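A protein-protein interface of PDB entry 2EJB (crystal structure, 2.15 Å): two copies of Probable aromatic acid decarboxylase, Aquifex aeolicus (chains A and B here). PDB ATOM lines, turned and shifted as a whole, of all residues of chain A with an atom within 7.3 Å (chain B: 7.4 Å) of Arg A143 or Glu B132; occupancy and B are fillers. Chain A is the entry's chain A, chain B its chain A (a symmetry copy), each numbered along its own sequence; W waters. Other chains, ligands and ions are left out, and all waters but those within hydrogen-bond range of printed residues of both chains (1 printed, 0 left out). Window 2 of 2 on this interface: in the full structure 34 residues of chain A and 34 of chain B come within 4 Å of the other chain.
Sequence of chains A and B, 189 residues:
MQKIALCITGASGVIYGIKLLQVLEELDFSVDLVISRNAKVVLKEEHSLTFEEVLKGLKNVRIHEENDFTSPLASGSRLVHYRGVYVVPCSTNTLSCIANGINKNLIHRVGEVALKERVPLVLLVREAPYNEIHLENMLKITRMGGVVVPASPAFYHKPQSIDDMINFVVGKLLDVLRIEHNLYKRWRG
Of the 10 printed residues of chain B, 4 touch a printed residue of chain A. Hydrophobic or aromatic side chains of chain A within 4 Å of the printed part of chain B: Leu A139. Among the printed residues, Asp or Glu carboxylates within 4 Å of a Lys or Arg side-chain nitrogen of the other chain: Arg A143 with Glu B132 and Arg A143 with Glu B136.
Water W1 lies within hydrogen-bond range of the side-chain hydroxyl (OG1) of Thr A142 (2.7 Å) and the backbone carbonyl oxygen (O) of Tyr B130 (2.8 Å).
Printed residues of chain B within 4 Å of Leu A139: Leu B135 (3.6 Å), Glu B136 (3.5 Å) and Leu B139 (3.98 Å). Arg A143 touches just these residues of chain B: Glu B132 and Glu B136. Of the printed residues of chain A, Glu B132 touches Thr A142 (3.6 Å) and Arg A143 (3.6 Å). Asn B137 touches none of the printed residues of chain A. Of the printed residues of chain A, Leu B139 touches Glu A136 (3.5 Å) and Leu A139 (3.98 Å). The nearest residue of chain A that does not touch Glu B132 is Leu A139 (4.03 Å).
The side-chain hydroxyl of Thr A142 sits at hydrogen-bond distance from the backbone carbonyl oxygen of Met A138 (2.7 Å).
The side-chain carboxylate (OE1) of Glu B132 is in salt-bridge range of the guanidinium group (NE) of Arg A143, at 3.6 Å. NH2 of Arg A143 lies within salt-bridge range of OE2 of Glu B136, 2.6 Å away.
Among the printed residues, pairs that only touch across the chains: Glu A136 with Leu B139, Leu A139 with Leu B135, Leu A139 with Glu B136, Leu A139 with Leu B139, Thr A142 with Glu B132 and Thr A142 with Leu B135.
Glu A136 touches Leu B139, and with the chains exchanged Leu A139 touches Glu B136. Leu B139 touches its own counterpart, Leu A139.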
ATOM      1  N   GLU A 136     -19.667   3.183 -11.374  1.00  0.00           N
ATOM      2  CA  GLU A 136     -18.992   1.927 -11.630  1.00  0.00           C
ATOM      3  C   GLU A 136     -18.881   1.619 -13.115  1.00  0.00           C
ATOM      4  O   GLU A 136     -17.895   1.032 -13.552  1.00  0.00           O
ATOM      5  CB  GLU A 136     -19.689   0.792 -10.873  1.00  0.00           C
ATOM      6  CG  GLU A 136     -19.412   0.853  -9.371  1.00  0.00           C
ATOM      7  CD  GLU A 136     -20.082  -0.261  -8.597  1.00  0.00           C
ATOM      8  OE1 GLU A 136     -21.328  -0.254  -8.501  1.00  0.00           O
ATOM      9  OE2 GLU A 136     -19.354  -1.145  -8.094  1.00  0.00           O
ATOM     10  N   ASN A 137     -19.880   2.016 -13.895  1.00  0.00           N
ATOM     11  CA  ASN A 137     -19.822   1.758 -15.328  1.00  0.00           C
ATOM     12  C   ASN A 137     -18.698   2.575 -15.935  1.00  0.00           C
ATOM     13  O   ASN A 137     -17.956   2.087 -16.785  1.00  0.00           O
ATOM     14  CB  ASN A 137     -21.149   2.120 -15.995  1.00  0.00           C
ATOM     15  CG  ASN A 137     -22.225   1.078 -15.750  1.00  0.00           C
ATOM     16  OD1 ASN A 137     -23.411   1.340 -15.930  1.00  0.00           O
ATOM     17  ND2 ASN A 137     -21.813  -0.109 -15.344  1.00  0.00           N
ATOM     18  N   MET A 138     -18.575   3.824 -15.497  1.00  0.00           N
ATOM     19  CA  MET A 138     -17.524   4.690 -16.011  1.00  0.00           C
ATOM     20  C   MET A 138     -16.162   4.166 -15.583  1.00  0.00           C
ATOM     21  O   MET A 138     -15.199   4.254 -16.334  1.00  0.00           O
ATOM     22  CB  MET A 138     -17.717   6.130 -15.519  1.00  0.00           C
ATOM     23  CG  MET A 138     -18.920   6.837 -16.145  1.00  0.00           C
ATOM     24  SD  MET A 138     -19.046   8.598 -15.728  1.00  0.00           S
ATOM     25  CE  MET A 138     -19.801   8.500 -14.135  1.00  0.00           C
ATOM     26  N   LEU A 139     -16.095   3.609 -14.377  1.00  0.00           N
ATOM     27  CA  LEU A 139     -14.848   3.070 -13.848  1.00  0.00           C
ATOM     28  C   LEU A 139     -14.420   1.854 -14.652  1.00  0.00           C
ATOM     29  O   LEU A 139     -13.239   1.678 -14.955  1.00  0.00           O
ATOM     30  CB  LEU A 139     -15.024   2.656 -12.387  1.00  0.00           C
ATOM     31  CG  LEU A 139     -14.104   3.281 -11.340  1.00  0.00           C
ATOM     32  CD1 LEU A 139     -14.304   2.542 -10.028  1.00  0.00           C
ATOM     33  CD2 LEU A 139     -12.648   3.202 -11.777  1.00  0.00           C
ATOM     34  N   LYS A 140     -15.385   1.000 -14.979  1.00  0.00           N
ATOM     35  CA  LYS A 140     -15.083  -0.189 -15.760  1.00  0.00           C
ATOM     36  C   LYS A 140     -14.579   0.221 -17.143  1.00  0.00           C
ATOM     37  O   LYS A 140     -13.586  -0.323 -17.623  1.00  0.00           O
ATOM     38  CB  LYS A 140     -16.315  -1.091 -15.883  1.00  0.00           C
ATOM     39  CG  LYS A 140     -16.062  -2.321 -16.739  1.00  0.00           C
ATOM     40  CD  LYS A 140     -16.524  -3.612 -16.089  1.00  0.00           C
ATOM     41  CE  LYS A 140     -15.996  -4.827 -16.862  1.00  0.00           C
ATOM     42  NZ  LYS A 140     -16.566  -6.121 -16.382  1.00  0.00           N
ATOM     43  N   ILE A 141     -15.256   1.177 -17.783  1.00  0.00           N
ATOM     44  CA  ILE A 141     -14.825   1.640 -19.108  1.00  0.00           C
ATOM     45  C   ILE A 141     -13.381   2.129 -19.002  1.00  0.00           C
ATOM     46  O   ILE A 141     -12.513   1.727 -19.779  1.00  0.00           O
ATOM     47  CB  ILE A 141     -15.681   2.832 -19.625  1.00  0.00           C
ATOM     48  CG1 ILE A 141     -17.119   2.385 -19.911  1.00  0.00           C
ATOM     49  CG2 ILE A 141     -15.034   3.437 -20.873  1.00  0.00           C
ATOM     50  CD1 ILE A 141     -17.234   1.258 -20.904  1.00  0.00           C
ATOM     51  N   THR A 142     -13.141   2.992 -18.017  1.00  0.00           N
ATOM     52  CA  THR A 142     -11.829   3.575 -17.780  1.00  0.00           C
ATOM     53  C   THR A 142     -10.736   2.527 -17.579  1.00  0.00           C
ATOM     54  O   THR A 142      -9.706   2.562 -18.248  1.00  0.00           O
ATOM     55  CB  THR A 142     -11.876   4.501 -16.558  1.00  0.00           C
ATOM     56  OG1 THR A 142     -12.835   5.538 -16.794  1.00  0.00           O
ATOM     57  CG2 THR A 142     -10.507   5.127 -16.295  1.00  0.00           C
ATOM     58  N   ARG A 143     -10.964   1.598 -16.657  1.00  0.00           N
ATOM     59  CA  ARG A 143      -9.989   0.550 -16.392  1.00  0.00           C
ATOM     60  C   ARG A 143      -9.722  -0.275 -17.641  1.00  0.00           C
ATOM     61  O   ARG A 143      -8.617  -0.782 -17.828  1.00  0.00           O
ATOM     62  CB  ARG A 143     -10.472  -0.343 -15.250  1.00  0.00           C
ATOM     63  CG  ARG A 143     -10.343   0.337 -13.903  1.00  0.00           C
ATOM     64  CD  ARG A 143     -11.073  -0.390 -12.793  1.00  0.00           C
ATOM     65  NE  ARG A 143     -10.777   0.204 -11.489  1.00  0.00           N
ATOM     66  CZ  ARG A 143     -11.426  -0.078 -10.361  1.00  0.00           C
ATOM     67  NH1 ARG A 143     -12.426  -0.949 -10.362  1.00  0.00           N
ATOM     68  NH2 ARG A 143     -11.058   0.497  -9.225  1.00  0.00           N
ATOM     69  N   MET A 144     -10.723  -0.394 -18.505  1.00  0.00           N
ATOM     70  CA  MET A 144     -10.559  -1.162 -19.731  1.00  0.00           C
ATOM     71  C   MET A 144      -9.802  -0.402 -20.814  1.00  0.00           C
ATOM     72  O   MET A 144      -9.601  -0.921 -21.913  1.00  0.00           O
ATOM     73  CB  MET A 144     -11.922  -1.618 -20.259  1.00  0.00           C
ATOM     74  CG  MET A 144     -12.494  -2.778 -19.471  1.00  0.00           C
ATOM     75  SD  MET A 144     -14.004  -3.411 -20.172  1.00  0.00           S
ATOM     76  CE  MET A 144     -13.348  -4.457 -21.525  1.00  0.00           C
ATOM     77  N   GLY A 145      -9.375   0.821 -20.504  1.00  0.00           N
ATOM     78  CA  GLY A 145      -8.630   1.602 -21.478  1.00  0.00           C
ATOM     79  C   GLY A 145      -9.445   2.700 -22.132  1.00  0.00           C
ATOM     80  O   GLY A 145      -8.896   3.570 -22.806  1.00  0.00           O
ATOM     81  N   GLY A 146     -10.761   2.656 -21.948  1.00  0.00           N
ATOM     82  CA  GLY A 146     -11.614   3.671 -22.533  1.00  0.00           C
ATOM     83  C   GLY A 146     -11.457   4.980 -21.785  1.00  0.00           C
ATOM     84  O   GLY A 146     -10.937   5.009 -20.668  1.00  0.00           O
ATOM     85  N   TYR B 130     -12.254  12.143 -16.642  1.00  0.00           N
ATOM     86  CA  TYR B 130     -12.113  11.565 -15.311  1.00  0.00           C
ATOM     87  C   TYR B 130     -11.043  10.478 -15.372  1.00  0.00           C
ATOM     88  O   TYR B 130     -10.943   9.751 -16.366  1.00  0.00           O
ATOM     89  CB  TYR B 130     -13.404  10.873 -14.841  1.00  0.00           C
ATOM     90  CG  TYR B 130     -14.614  11.742 -14.572  1.00  0.00           C
ATOM     91  CD1 TYR B 130     -14.502  12.946 -13.882  1.00  0.00           C
ATOM     92  CD2 TYR B 130     -15.888  11.316 -14.949  1.00  0.00           C
ATOM     93  CE1 TYR B 130     -15.628  13.707 -13.578  1.00  0.00           C
ATOM     94  CE2 TYR B 130     -17.023  12.066 -14.646  1.00  0.00           C
ATOM     95  CZ  TYR B 130     -16.883  13.259 -13.959  1.00  0.00           C
ATOM     96  OH  TYR B 130     -17.994  14.010 -13.656  1.00  0.00           O
ATOM     97  N   ASN B 131     -10.239  10.358 -14.321  1.00  0.00           N
ATOM     98  CA  ASN B 131      -9.271   9.271 -14.280  1.00  0.00           C
ATOM     99  C   ASN B 131      -9.888   8.325 -13.257  1.00  0.00           C
ATOM    100  O   ASN B 131     -10.936   8.649 -12.684  1.00  0.00           O
ATOM    101  CB  ASN B 131      -7.860   9.741 -13.859  1.00  0.00           C
ATOM    102  CG  ASN B 131      -7.802  10.316 -12.445  1.00  0.00           C
ATOM    103  OD1 ASN B 131      -8.509   9.873 -11.543  1.00  0.00           O
ATOM    104  ND2 ASN B 131      -6.923  11.296 -12.248  1.00  0.00           N
ATOM    105  N   GLU B 132      -9.280   7.165 -13.036  1.00  0.00           N
ATOM    106  CA  GLU B 132      -9.816   6.200 -12.077  1.00  0.00           C
ATOM    107  C   GLU B 132      -9.956   6.758 -10.667  1.00  0.00           C
ATOM    108  O   GLU B 132     -10.914   6.446  -9.975  1.00  0.00           O
ATOM    109  CB  GLU B 132      -8.939   4.944 -12.023  1.00  0.00           C
ATOM    110  CG  GLU B 132      -9.000   4.074 -13.258  1.00  0.00           C
ATOM    111  CD  GLU B 132      -7.971   2.967 -13.229  1.00  0.00           C
ATOM    112  OE1 GLU B 132      -7.890   2.260 -12.200  1.00  0.00           O
ATOM    113  OE2 GLU B 132      -7.245   2.815 -14.231  1.00  0.00           O
ATOM    114  N   ILE B 133      -8.998   7.572 -10.238  1.00  0.00           N
ATOM    115  CA  ILE B 133      -9.055   8.140  -8.892  1.00  0.00           C
ATOM    116  C   ILE B 133     -10.301   8.997  -8.701  1.00  0.00           C
ATOM    117  O   ILE B 133     -10.988   8.891  -7.678  1.00  0.00           O
ATOM    118  CB  ILE B 133      -7.808   8.994  -8.587  1.00  0.00           C
ATOM    119  CG1 ILE B 133      -6.546   8.132  -8.706  1.00  0.00           C
ATOM    120  CG2 ILE B 133      -7.907   9.577  -7.173  1.00  0.00           C
ATOM    121  CD1 ILE B 133      -5.253   8.925  -8.578  1.00  0.00           C
ATOM    122  N   HIS B 134     -10.592   9.840  -9.687  1.00  0.00           N
ATOM    123  CA  HIS B 134     -11.765  10.709  -9.628  1.00  0.00           C
ATOM    124  C   HIS B 134     -13.018   9.860  -9.445  1.00  0.00           C
ATOM    125  O   HIS B 134     -13.870  10.160  -8.602  1.00  0.00           O
ATOM    126  CB  HIS B 134     -11.889  11.522 -10.925  1.00  0.00           C
ATOM    127  CG  HIS B 134     -10.749  12.468 -11.162  1.00  0.00           C
ATOM    128  ND1 HIS B 134     -10.307  12.797 -12.423  1.00  0.00           N
ATOM    129  CD2 HIS B 134      -9.960  13.144 -10.293  1.00  0.00           C
ATOM    130  CE1 HIS B 134      -9.285  13.633 -12.324  1.00  0.00           C
ATOM    131  NE2 HIS B 134      -9.057  13.859 -11.044  1.00  0.00           N
ATOM    132  N   LEU B 135     -13.120   8.797 -10.241  1.00  0.00           N
ATOM    133  CA  LEU B 135     -14.269   7.899 -10.194  1.00  0.00           C
ATOM    134  C   LEU B 135     -14.414   7.183  -8.863  1.00  0.00           C
ATOM    135  O   LEU B 135     -15.510   7.088  -8.311  1.00  0.00           O
ATOM    136  CB  LEU B 135     -14.193   6.841 -11.310  1.00  0.00           C
ATOM    137  CG  LEU B 135     -14.665   7.140 -12.742  1.00  0.00           C
ATOM    138  CD1 LEU B 135     -15.651   8.302 -12.746  1.00  0.00           C
ATOM    139  CD2 LEU B 135     -13.485   7.426 -13.633  1.00  0.00           C
ATOM    140  N   GLU B 136     -13.313   6.662  -8.347  1.00  0.00           N
ATOM    141  CA  GLU B 136     -13.382   5.942  -7.092  1.00  0.00           C
ATOM    142  C   GLU B 136     -13.679   6.856  -5.913  1.00  0.00           C
ATOM    143  O   GLU B 136     -14.361   6.453  -4.975  1.00  0.00           O
ATOM    144  CB  GLU B 136     -12.093   5.144  -6.871  1.00  0.00           C
ATOM    145  CG  GLU B 136     -12.014   3.923  -7.785  1.00  0.00           C
ATOM    146  CD  GLU B 136     -10.754   3.110  -7.585  1.00  0.00           C
ATOM    147  OE1 GLU B 136      -9.662   3.607  -7.937  1.00  0.00           O
ATOM    148  OE2 GLU B 136     -10.864   1.976  -7.068  1.00  0.00           O
ATOM    149  N   ASN B 137     -13.178   8.086  -5.956  1.00  0.00           N
ATOM    150  CA  ASN B 137     -13.440   9.010  -4.860  1.00  0.00           C
ATOM    151  C   ASN B 137     -14.919   9.347  -4.837  1.00  0.00           C
ATOM    152  O   ASN B 137     -15.531   9.412  -3.773  1.00  0.00           O
ATOM    153  CB  ASN B 137     -12.616  10.287  -5.021  1.00  0.00           C
ATOM    154  CG  ASN B 137     -11.160  10.089  -4.640  1.00  0.00           C
ATOM    155  OD1 ASN B 137     -10.299  10.889  -4.997  1.00  0.00           O
ATOM    156  ND2 ASN B 137     -10.883   9.026  -3.907  1.00  0.00           N
ATOM    157  N   MET B 138     -15.491   9.565  -6.017  1.00  0.00           N
ATOM    158  CA  MET B 138     -16.907   9.889  -6.105  1.00  0.00           C
ATOM    159  C   MET B 138     -17.743   8.698  -5.665  1.00  0.00           C
ATOM    160  O   MET B 138     -18.785   8.867  -5.044  1.00  0.00           O
ATOM    161  CB  MET B 138     -17.282  10.303  -7.534  1.00  0.00           C
ATOM    162  CG  MET B 138     -16.711  11.659  -7.951  1.00  0.00           C
ATOM    163  SD  MET B 138     -17.306  12.252  -9.560  1.00  0.00           S
ATOM    164  CE  MET B 138     -16.246  11.353 -10.649  1.00  0.00           C
ATOM    165  N   LEU B 139     -17.271   7.496  -5.981  1.00  0.00           N
ATOM    166  CA  LEU B 139     -17.978   6.273  -5.619  1.00  0.00           C
ATOM    167  C   LEU B 139     -17.979   6.096  -4.110  1.00  0.00           C
ATOM    168  O   LEU B 139     -18.986   5.702  -3.519  1.00  0.00           O
ATOM    169  CB  LEU B 139     -17.302   5.058  -6.256  1.00  0.00           C
ATOM    170  CG  LEU B 139     -18.138   4.158  -7.164  1.00  0.00           C
ATOM    171  CD1 LEU B 139     -17.329   2.908  -7.470  1.00  0.00           C
ATOM    172  CD2 LEU B 139     -19.456   3.786  -6.498  1.00  0.00           C
HETATM  173  O   HOH W   1     -11.863   7.733 -18.123  1.00  0.00           O
